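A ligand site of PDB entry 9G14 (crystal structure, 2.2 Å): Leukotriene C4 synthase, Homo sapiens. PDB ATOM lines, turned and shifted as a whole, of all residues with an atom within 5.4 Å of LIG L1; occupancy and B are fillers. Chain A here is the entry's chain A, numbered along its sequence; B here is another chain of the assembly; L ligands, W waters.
OH of Tyr 100 is in hydrogen-bond range of O4 of LIG L1 (2.5 Å). O of Ser 30 of chain B sits at hydrogen-bond distance from N1 of LIG L1. The side-chain hydroxyl of Ser 30 of chain B lies within hydrogen-bond range of an oxygen (O2) of LIG L1 (2.9 Å). The guanidinium group (NE) of Arg 58 lies within salt-bridge range of an oxygen (O5) of LIG L1. An oxygen (O4) of LIG L1 lies within hydrogen-bond range of the guanidinium group (NE) of Arg 111 (3.0 Å). O1 of LIG L1 lies within hydrogen-bond range of NE2 of Gln 60 of chain B, 3.2 Å away. An oxygen (O6) of LIG L1 is in salt-bridge range of the guanidinium group (NH1) of Arg 37 of chain B, at 3.3 Å. A nitrogen (N2) of LIG L1 lies close to the side-chain amide nitrogen of Asn 62, at 3.4 Å.
OH of Tyr 100 lies close to OD1 of Asn 62. The side-chain hydroxyl (OG) of Ser 30 of chain B lies within hydrogen-bond range of the side-chain hydroxyl (OH) of Tyr 66 (3.2 Å). O of Arg 58 sits close to OD1 of Asn 62, 3.0 Å away. The guanidinium group (NH1) of Arg 58 lies within hydrogen-bond range of the side-chain hydroxyl (OH) of Tyr 57 of chain B, 3.0 Å away. The guanidinium group (NH2) of Arg 37 of chain B lies within hydrogen-bond range of the backbone carbonyl oxygen (O) of Leu 46 of chain B (2.7 Å).
OH of Tyr 66 touches C3 of LIG L1, 3.4 Å away. Tyr 104 touches LIG L1. Leu 115 touches LIG L1. CB of Val 33 of chain B touches N1 of LIG L1, at 3.5 Å. Ile 34 of chain B touches LIG L1. Pro 44 of chain B touches LIG L1. Pro 45 of chain B touches LIG L1 (CA to O5, 3.7 Å). 14 residues have an atom within 4 Å of LIG L1: Arg 58, Asn 62, Tyr 66, Tyr 100, Tyr 104, Arg 111, Leu 115, Ser 30 of chain B, Val 33 of chain B, Ile 34 of chain B, Arg 37 of chain B, Pro 44 of chain B, Pro 45 of chain B and Gln 60 of chain B. The nearest printed residue that does not touch LIG L1 is Thr 47 of chain B (4.4 Å).
Water W2 lies within hydrogen-bond range of a nitrogen (N1) of LIG L1 (2.5 Å) and the guanidinium group (NE) of Arg 37 of chain B (3.0 Å). Water W3 lies within hydrogen-bond range of the side-chain carboxylate of Glu 65 (2.6 Å), an oxygen (O2) of LIG L1 (2.6 Å) and the side-chain amide oxygen of Gln 60 of chain B (3.1 Å). Water W1 bridges O6 of LIG L1 and NH1 of Arg 37 of chain B.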
ATOM      1  N   ARG A  58      33.346  23.031 -19.150  1.00  0.00           N
ATOM      2  CA  ARG A  58      32.408  21.899 -19.062  1.00  0.00           C
ATOM      3  C   ARG A  58      32.136  21.290 -20.438  1.00  0.00           C
ATOM      4  O   ARG A  58      31.907  20.080 -20.525  1.00  0.00           O
ATOM      5  CB  ARG A  58      31.070  22.306 -18.399  1.00  0.00           C
ATOM      6  CG  ARG A  58      31.160  22.570 -16.884  1.00  0.00           C
ATOM      7  CD  ARG A  58      31.725  21.435 -16.055  1.00  0.00           C
ATOM      8  NE  ARG A  58      31.036  20.185 -16.322  1.00  0.00           N
ATOM      9  CZ  ARG A  58      31.535  18.979 -16.067  1.00  0.00           C
ATOM     10  NH1 ARG A  58      32.710  18.853 -15.452  1.00  0.00           N
ATOM     11  NH2 ARG A  58      30.846  17.887 -16.377  1.00  0.00           N
ATOM     12  N   ASN A  62      32.924  17.336 -21.290  1.00  0.00           N
ATOM     13  CA  ASN A  62      31.891  16.501 -21.872  1.00  0.00           C
ATOM     14  C   ASN A  62      32.358  15.863 -23.163  1.00  0.00           C
ATOM     15  O   ASN A  62      32.118  14.679 -23.380  1.00  0.00           O
ATOM     16  CB  ASN A  62      30.631  17.313 -22.133  1.00  0.00           C
ATOM     17  CG  ASN A  62      29.660  17.270 -20.997  1.00  0.00           C
ATOM     18  OD1 ASN A  62      29.552  18.207 -20.192  1.00  0.00           O
ATOM     19  ND2 ASN A  62      28.886  16.181 -20.956  1.00  0.00           N
ATOM     20  N   GLU A  65      34.973  13.054 -22.253  1.00  0.00           N
ATOM     21  CA  GLU A  65      34.375  11.880 -21.626  1.00  0.00           C
ATOM     22  C   GLU A  65      33.620  10.987 -22.624  1.00  0.00           C
ATOM     23  O   GLU A  65      33.590   9.777 -22.496  1.00  0.00           O
ATOM     24  CB  GLU A  65      33.489  12.318 -20.458  1.00  0.00           C
ATOM     25  CG  GLU A  65      34.332  12.764 -19.276  1.00  0.00           C
ATOM     26  CD  GLU A  65      33.591  13.132 -18.007  1.00  0.00           C
ATOM     27  OE1 GLU A  65      32.342  13.196 -18.052  1.00  0.00           O
ATOM     28  OE2 GLU A  65      34.260  13.352 -16.962  1.00  0.00           O
ATOM     29  N   TYR A  66      33.029  11.606 -23.632  1.00  0.00           N
ATOM     30  CA  TYR A  66      32.311  10.944 -24.695  1.00  0.00           C
ATOM     31  C   TYR A  66      33.217  10.496 -25.839  1.00  0.00           C
ATOM     32  O   TYR A  66      32.787   9.667 -26.618  1.00  0.00           O
ATOM     33  CB  TYR A  66      31.205  11.867 -25.201  1.00  0.00           C
ATOM     34  CG  TYR A  66      29.941  11.742 -24.398  1.00  0.00           C
ATOM     35  CD1 TYR A  66      29.747  12.460 -23.229  1.00  0.00           C
ATOM     36  CD2 TYR A  66      28.924  10.904 -24.822  1.00  0.00           C
ATOM     37  CE1 TYR A  66      28.586  12.343 -22.497  1.00  0.00           C
ATOM     38  CE2 TYR A  66      27.749  10.778 -24.093  1.00  0.00           C
ATOM     39  CZ  TYR A  66      27.593  11.480 -22.931  1.00  0.00           C
ATOM     40  OH  TYR A  66      26.424  11.330 -22.227  1.00  0.00           O
ATOM     41  N   TYR A 100      27.983  21.808 -30.566  1.00  0.00           N
ATOM     42  CA  TYR A 100      27.631  21.746 -29.145  1.00  0.00           C
ATOM     43  C   TYR A 100      28.603  22.615 -28.347  1.00  0.00           C
ATOM     44  O   TYR A 100      28.191  23.333 -27.431  1.00  0.00           O
ATOM     45  CB  TYR A 100      27.666  20.264 -28.666  1.00  0.00           C
ATOM     46  CG  TYR A 100      27.837  20.078 -27.175  1.00  0.00           C
ATOM     47  CD1 TYR A 100      26.771  20.239 -26.304  1.00  0.00           C
ATOM     48  CD2 TYR A 100      29.078  19.781 -26.636  1.00  0.00           C
ATOM     49  CE1 TYR A 100      26.929  20.101 -24.932  1.00  0.00           C
ATOM     50  CE2 TYR A 100      29.263  19.669 -25.266  1.00  0.00           C
ATOM     51  CZ  TYR A 100      28.181  19.809 -24.421  1.00  0.00           C
ATOM     52  OH  TYR A 100      28.352  19.657 -23.064  1.00  0.00           O
ATOM     53  N   TYR A 104      27.487  26.055 -26.414  1.00  0.00           N
ATOM     54  CA  TYR A 104      27.731  26.066 -24.968  1.00  0.00           C
ATOM     55  C   TYR A 104      28.601  27.256 -24.573  1.00  0.00           C
ATOM     56  O   TYR A 104      28.334  27.896 -23.554  1.00  0.00           O
ATOM     57  CB  TYR A 104      28.411  24.748 -24.515  1.00  0.00           C
ATOM     58  CG  TYR A 104      28.155  24.329 -23.075  1.00  0.00           C
ATOM     59  CD1 TYR A 104      27.543  25.194 -22.172  1.00  0.00           C
ATOM     60  CD2 TYR A 104      28.551  23.080 -22.614  1.00  0.00           C
ATOM     61  CE1 TYR A 104      27.344  24.834 -20.850  1.00  0.00           C
ATOM     62  CE2 TYR A 104      28.355  22.711 -21.282  1.00  0.00           C
ATOM     63  CZ  TYR A 104      27.742  23.593 -20.412  1.00  0.00           C
ATOM     64  OH  TYR A 104      27.506  23.256 -19.108  1.00  0.00           O
ATOM     65  N   ARG A 111      23.500  25.080 -26.214  1.00  0.00           N
ATOM     66  CA  ARG A 111      24.192  23.804 -26.312  1.00  0.00           C
ATOM     67  C   ARG A 111      23.186  22.651 -26.557  1.00  0.00           C
ATOM     68  O   ARG A 111      23.591  21.619 -27.065  1.00  0.00           O
ATOM     69  CB  ARG A 111      25.042  23.539 -25.037  1.00  0.00           C
ATOM     70  CG  ARG A 111      24.434  22.569 -24.007  1.00  0.00           C
ATOM     71  CD  ARG A 111      24.955  22.691 -22.588  1.00  0.00           C
ATOM     72  NE  ARG A 111      24.277  21.719 -21.736  1.00  0.00           N
ATOM     73  CZ  ARG A 111      23.234  21.998 -20.961  1.00  0.00           C
ATOM     74  NH1 ARG A 111      22.659  21.044 -20.258  1.00  0.00           N
ATOM     75  NH2 ARG A 111      22.760  23.241 -20.887  1.00  0.00           N
ATOM     76  N   LEU A 115      23.483  19.158 -28.765  1.00  0.00           N
ATOM     77  CA  LEU A 115      23.687  18.054 -27.834  1.00  0.00           C
ATOM     78  C   LEU A 115      22.719  16.925 -28.176  1.00  0.00           C
ATOM     79  O   LEU A 115      23.124  15.760 -28.189  1.00  0.00           O
ATOM     80  CB  LEU A 115      23.460  18.536 -26.393  1.00  0.00           C
ATOM     81  CG  LEU A 115      23.408  17.476 -25.311  1.00  0.00           C
ATOM     82  CD1 LEU A 115      24.756  16.792 -25.154  1.00  0.00           C
ATOM     83  CD2 LEU A 115      22.902  18.061 -24.009  1.00  0.00           C
ATOM     84  N   PHE B  29      24.618   5.594 -16.702  1.00  0.00           N
ATOM     85  CA  PHE B  29      25.224   6.450 -15.676  1.00  0.00           C
ATOM     86  C   PHE B  29      24.948   7.936 -15.975  1.00  0.00           C
ATOM     87  O   PHE B  29      24.707   8.712 -15.053  1.00  0.00           O
ATOM     88  CB  PHE B  29      26.732   6.202 -15.598  1.00  0.00           C
ATOM     89  CG  PHE B  29      27.138   4.834 -15.113  1.00  0.00           C
ATOM     90  CD1 PHE B  29      26.302   4.093 -14.288  1.00  0.00           C
ATOM     91  CD2 PHE B  29      28.364   4.289 -15.450  1.00  0.00           C
ATOM     92  CE1 PHE B  29      26.683   2.836 -13.830  1.00  0.00           C
ATOM     93  CE2 PHE B  29      28.742   3.044 -14.980  1.00  0.00           C
ATOM     94  CZ  PHE B  29      27.914   2.334 -14.150  1.00  0.00           C
ATOM     95  N   SER B  30      24.998   8.310 -17.260  1.00  0.00           N
ATOM     96  CA  SER B  30      24.688   9.659 -17.723  1.00  0.00           C
ATOM     97  C   SER B  30      23.217  10.000 -17.492  1.00  0.00           C
ATOM     98  O   SER B  30      22.898  11.149 -17.186  1.00  0.00           O
ATOM     99  CB  SER B  30      25.001   9.780 -19.206  1.00  0.00           C
ATOM    100  OG  SER B  30      26.392   9.944 -19.385  1.00  0.00           O
ATOM    101  N   LEU B  31      22.312   9.016 -17.661  1.00  0.00           N
ATOM    102  CA  LEU B  31      20.884   9.198 -17.440  1.00  0.00           C
ATOM    103  C   LEU B  31      20.621   9.487 -15.949  1.00  0.00           C
ATOM    104  O   LEU B  31      19.807  10.350 -15.626  1.00  0.00           O
ATOM    105  CB  LEU B  31      20.108   7.956 -17.899  1.00  0.00           C
ATOM    106  CG  LEU B  31      18.582   8.002 -17.736  1.00  0.00           C
ATOM    107  CD1 LEU B  31      17.970   9.019 -18.668  1.00  0.00           C
ATOM    108  CD2 LEU B  31      17.976   6.631 -17.990  1.00  0.00           C
ATOM    109  N   VAL B  33      22.726  10.955 -13.816  1.00  0.00           N
ATOM    110  CA  VAL B  33      23.243  12.286 -13.495  1.00  0.00           C
ATOM    111  C   VAL B  33      22.229  13.363 -13.964  1.00  0.00           C
ATOM    112  O   VAL B  33      22.029  14.361 -13.263  1.00  0.00           O
ATOM    113  CB  VAL B  33      24.671  12.490 -14.048  1.00  0.00           C
ATOM    114  CG1 VAL B  33      25.124  13.942 -13.891  1.00  0.00           C
ATOM    115  CG2 VAL B  33      25.647  11.556 -13.358  1.00  0.00           C
ATOM    116  N   ILE B  34      21.537  13.116 -15.096  1.00  0.00           N
ATOM    117  CA  ILE B  34      20.496  14.021 -15.598  1.00  0.00           C
ATOM    118  C   ILE B  34      19.317  14.038 -14.622  1.00  0.00           C
ATOM    119  O   ILE B  34      18.799  15.113 -14.306  1.00  0.00           O
ATOM    120  CB  ILE B  34      20.071  13.600 -17.023  1.00  0.00           C
ATOM    121  CG1 ILE B  34      21.221  13.799 -18.009  1.00  0.00           C
ATOM    122  CG2 ILE B  34      18.835  14.364 -17.480  1.00  0.00           C
ATOM    123  CD1 ILE B  34      21.000  13.134 -19.372  1.00  0.00           C
ATOM    124  N   ARG B  37      20.323  16.044 -11.559  1.00  0.00           N
ATOM    125  CA  ARG B  37      20.367  17.487 -11.851  1.00  0.00           C
ATOM    126  C   ARG B  37      18.988  18.135 -11.669  1.00  0.00           C
ATOM    127  O   ARG B  37      18.900  19.262 -11.195  1.00  0.00           O
ATOM    128  CB  ARG B  37      20.865  17.732 -13.274  1.00  0.00           C
ATOM    129  CG  ARG B  37      22.360  17.636 -13.387  1.00  0.00           C
ATOM    130  CD  ARG B  37      22.894  18.306 -14.619  1.00  0.00           C
ATOM    131  NE  ARG B  37      24.351  18.225 -14.649  1.00  0.00           N
ATOM    132  CZ  ARG B  37      25.168  19.142 -14.135  1.00  0.00           C
ATOM    133  NH1 ARG B  37      26.480  18.975 -14.202  1.00  0.00           N
ATOM    134  NH2 ARG B  37      24.679  20.234 -13.569  1.00  0.00           N
ATOM    135  N   PRO B  44      23.499  22.870 -15.367  1.00  0.00           N
ATOM    136  CA  PRO B  44      24.813  23.080 -16.000  1.00  0.00           C
ATOM    137  C   PRO B  44      25.092  24.566 -16.261  1.00  0.00           C
ATOM    138  O   PRO B  44      24.153  25.328 -16.483  1.00  0.00           O
ATOM    139  CB  PRO B  44      24.685  22.307 -17.312  1.00  0.00           C
ATOM    140  CG  PRO B  44      23.617  21.335 -17.062  1.00  0.00           C
ATOM    141  CD  PRO B  44      22.635  22.021 -16.206  1.00  0.00           C
ATOM    142  N   PRO B  45      26.359  25.023 -16.177  1.00  0.00           N
ATOM    143  CA  PRO B  45      27.599  24.247 -15.976  1.00  0.00           C
ATOM    144  C   PRO B  45      27.987  23.881 -14.543  1.00  0.00           C
ATOM    145  O   PRO B  45      29.144  23.547 -14.317  1.00  0.00           O
ATOM    146  CB  PRO B  45      28.654  25.166 -16.593  1.00  0.00           C
ATOM    147  CG  PRO B  45      28.153  26.542 -16.293  1.00  0.00           C
ATOM    148  CD  PRO B  45      26.656  26.444 -16.444  1.00  0.00           C
ATOM    149  N   LEU B  46      27.055  23.924 -13.575  1.00  0.00           N
ATOM    150  CA  LEU B  46      27.381  23.623 -12.183  1.00  0.00           C
ATOM    151  C   LEU B  46      27.594  22.147 -11.877  1.00  0.00           C
ATOM    152  O   LEU B  46      26.768  21.331 -12.237  1.00  0.00           O
ATOM    153  CB  LEU B  46      26.328  24.210 -11.221  1.00  0.00           C
ATOM    154  CG  LEU B  46      26.305  25.729 -11.132  1.00  0.00           C
ATOM    155  CD1 LEU B  46      25.115  26.207 -10.300  1.00  0.00           C
ATOM    156  CD2 LEU B  46      27.609  26.251 -10.560  1.00  0.00           C
ATOM    157  N   THR B  47      28.709  21.811 -11.210  1.00  0.00           N
ATOM    158  CA  THR B  47      28.989  20.418 -10.819  1.00  0.00           C
ATOM    159  C   THR B  47      28.992  20.208  -9.291  1.00  0.00           C
ATOM    160  O   THR B  47      28.991  19.064  -8.837  1.00  0.00           O
ATOM    161  CB  THR B  47      30.263  19.879 -11.466  1.00  0.00           C
ATOM    162  OG1 THR B  47      31.418  20.418 -10.836  1.00  0.00           O
ATOM    163  CG2 THR B  47      30.308  20.128 -12.953  1.00  0.00           C
ATOM    164  N   TYR B  57      27.427  12.244  -9.321  1.00  0.00           N
ATOM    165  CA  TYR B  57      28.246  12.948 -10.291  1.00  0.00           C
ATOM    166  C   TYR B  57      29.680  12.398 -10.272  1.00  0.00           C
ATOM    167  O   TYR B  57      30.232  12.122 -11.336  1.00  0.00           O
ATOM    168  CB  TYR B  57      28.195  14.473 -10.023  1.00  0.00           C
ATOM    169  CG  TYR B  57      29.222  15.230 -10.828  1.00  0.00           C
ATOM    170  CD1 TYR B  57      29.081  15.396 -12.200  1.00  0.00           C
ATOM    171  CD2 TYR B  57      30.383  15.703 -10.230  1.00  0.00           C
ATOM    172  CE1 TYR B  57      30.062  16.024 -12.954  1.00  0.00           C
ATOM    173  CE2 TYR B  57      31.376  16.320 -10.978  1.00  0.00           C
ATOM    174  CZ  TYR B  57      31.215  16.480 -12.340  1.00  0.00           C
ATOM    175  OH  TYR B  57      32.176  17.135 -13.052  1.00  0.00           O
ATOM    176  N   GLN B  60      29.853   8.819 -11.741  1.00  0.00           N
ATOM    177  CA  GLN B  60      29.819   8.850 -13.188  1.00  0.00           C
ATOM    178  C   GLN B  60      31.195   9.245 -13.739  1.00  0.00           C
ATOM    179  O   GLN B  60      31.660   8.619 -14.675  1.00  0.00           O
ATOM    180  CB  GLN B  60      28.722   9.819 -13.646  1.00  0.00           C
ATOM    181  CG  GLN B  60      28.524   9.896 -15.151  1.00  0.00           C
ATOM    182  CD  GLN B  60      29.375  10.971 -15.792  1.00  0.00           C
ATOM    183  OE1 GLN B  60      30.079  10.733 -16.786  1.00  0.00           O
ATOM    184  NE2 GLN B  60      29.356  12.172 -15.222  1.00  0.00           N
HETATM  185  N1  LIG L   1      24.551  13.629 -17.334  1.00  0.00           N
HETATM  186  C1  LIG L   1      25.422  12.840 -18.242  1.00  0.00           C
HETATM  187  C2  LIG L   1      26.892  13.003 -17.838  1.00  0.00           C
HETATM  188  O1  LIG L   1      27.144  13.740 -16.848  1.00  0.00           O
HETATM  189  O2  LIG L   1      27.743  12.367 -18.513  1.00  0.00           O
HETATM  190  C3  LIG L   1      25.119  13.159 -19.712  1.00  0.00           C
HETATM  191  C4  LIG L   1      25.938  14.305 -20.309  1.00  0.00           C
HETATM  192  C5  LIG L   1      25.077  15.458 -20.744  1.00  0.00           C
HETATM  193  O3  LIG L   1      24.001  15.292 -21.312  1.00  0.00           O
HETATM  194  N2  LIG L   1      25.546  16.663 -20.426  1.00  0.00           N
HETATM  195  C6  LIG L   1      24.965  17.902 -20.921  1.00  0.00           C
HETATM  196  C7  LIG L   1      25.917  19.042 -20.595  1.00  0.00           C
HETATM  197  O4  LIG L   1      26.433  19.694 -21.496  1.00  0.00           O
HETATM  198  C8  LIG L   1      23.549  18.119 -20.398  1.00  0.00           C
HETATM  199  S1  LIG L   1      23.402  18.147 -18.592  1.00  0.00           S
HETATM  200  N3  LIG L   1      26.194  19.234 -19.297  1.00  0.00           N
HETATM  201  C9  LIG L   1      27.133  20.212 -18.811  1.00  0.00           C
HETATM  202  C10 LIG L   1      27.721  19.796 -17.481  1.00  0.00           C
HETATM  203  O5  LIG L   1      28.192  20.658 -16.724  1.00  0.00           O
HETATM  204  O6  LIG L   1      27.707  18.567 -17.238  1.00  0.00           O
HETATM  205  C1  LG2 L   2      19.210   3.910 -21.062  1.00  0.00           C
HETATM  206  C2  LG2 L   2      17.933   3.933 -21.634  1.00  0.00           C
HETATM  207  C3  LG2 L   2      17.424   5.127 -22.172  1.00  0.00           C
HETATM  208  C4  LG2 L   2      20.186  10.909 -22.680  1.00  0.00           C
HETATM  209  C5  LG2 L   2      21.195  11.010 -23.881  1.00  0.00           C
HETATM  210  C6  LG2 L   2      22.720  10.719 -23.555  1.00  0.00           C
HETATM  211  C7  LG2 L   2      22.847   9.585 -22.464  1.00  0.00           C
HETATM  212  C8  LG2 L   2      21.830   9.684 -21.292  1.00  0.00           C
HETATM  213  C9  LG2 L   2      24.390  11.254 -25.371  1.00  0.00           C
HETATM  214  C10 LG2 L   2      24.636  12.667 -24.848  1.00  0.00           C
HETATM  215  C11 LG2 L   2      23.532  13.179 -23.892  1.00  0.00           C
HETATM  216  C12 LG2 L   2      23.229  12.043 -22.886  1.00  0.00           C
HETATM  217  C13 LG2 L   2      23.378   9.044 -25.452  1.00  0.00           C
HETATM  218  C14 LG2 L   2      24.456   7.983 -25.190  1.00  0.00           C
HETATM  219  C15 LG2 L   2      24.460   6.766 -25.908  1.00  0.00           C
HETATM  220  C16 LG2 L   2      25.423   5.790 -25.664  1.00  0.00           C
HETATM  221  C17 LG2 L   2      26.437   6.030 -24.728  1.00  0.00           C
HETATM  222  C18 LG2 L   2      26.473   7.240 -24.018  1.00  0.00           C
HETATM  223  C19 LG2 L   2      25.478   8.212 -24.257  1.00  0.00           C
HETATM  224  C20 LG2 L   2      18.205   6.283 -22.153  1.00  0.00           C
HETATM  225  C21 LG2 L   2      19.468   6.261 -21.585  1.00  0.00           C
HETATM  226  C22 LG2 L   2      19.983   5.090 -21.019  1.00  0.00           C
HETATM  227  N1  LG2 L   2      17.722   7.448 -22.646  1.00  0.00           N
HETATM  228  C23 LG2 L   2      18.467   8.577 -22.642  1.00  0.00           C
HETATM  229  C24 LG2 L   2      19.731   8.570 -22.031  1.00  0.00           C
HETATM  230  N2  LG2 L   2      20.199   7.396 -21.542  1.00  0.00           N
HETATM  231  N3  LG2 L   2      20.535   9.678 -21.965  1.00  0.00           N
HETATM  232  N4  LG2 L   2      23.541  10.356 -24.774  1.00  0.00           N
HETATM  233  O1  LG2 L   2      25.025  11.002 -26.386  1.00  0.00           O
HETATM  234  O   HOH W   1      26.796  16.511 -15.781  1.00  0.00           O
HETATM  235  O   HOH W   2      24.341  16.009 -16.653  1.00  0.00           O
HETATM  236  O   HOH W   3      30.224  12.402 -19.354  1.00  0.00           O
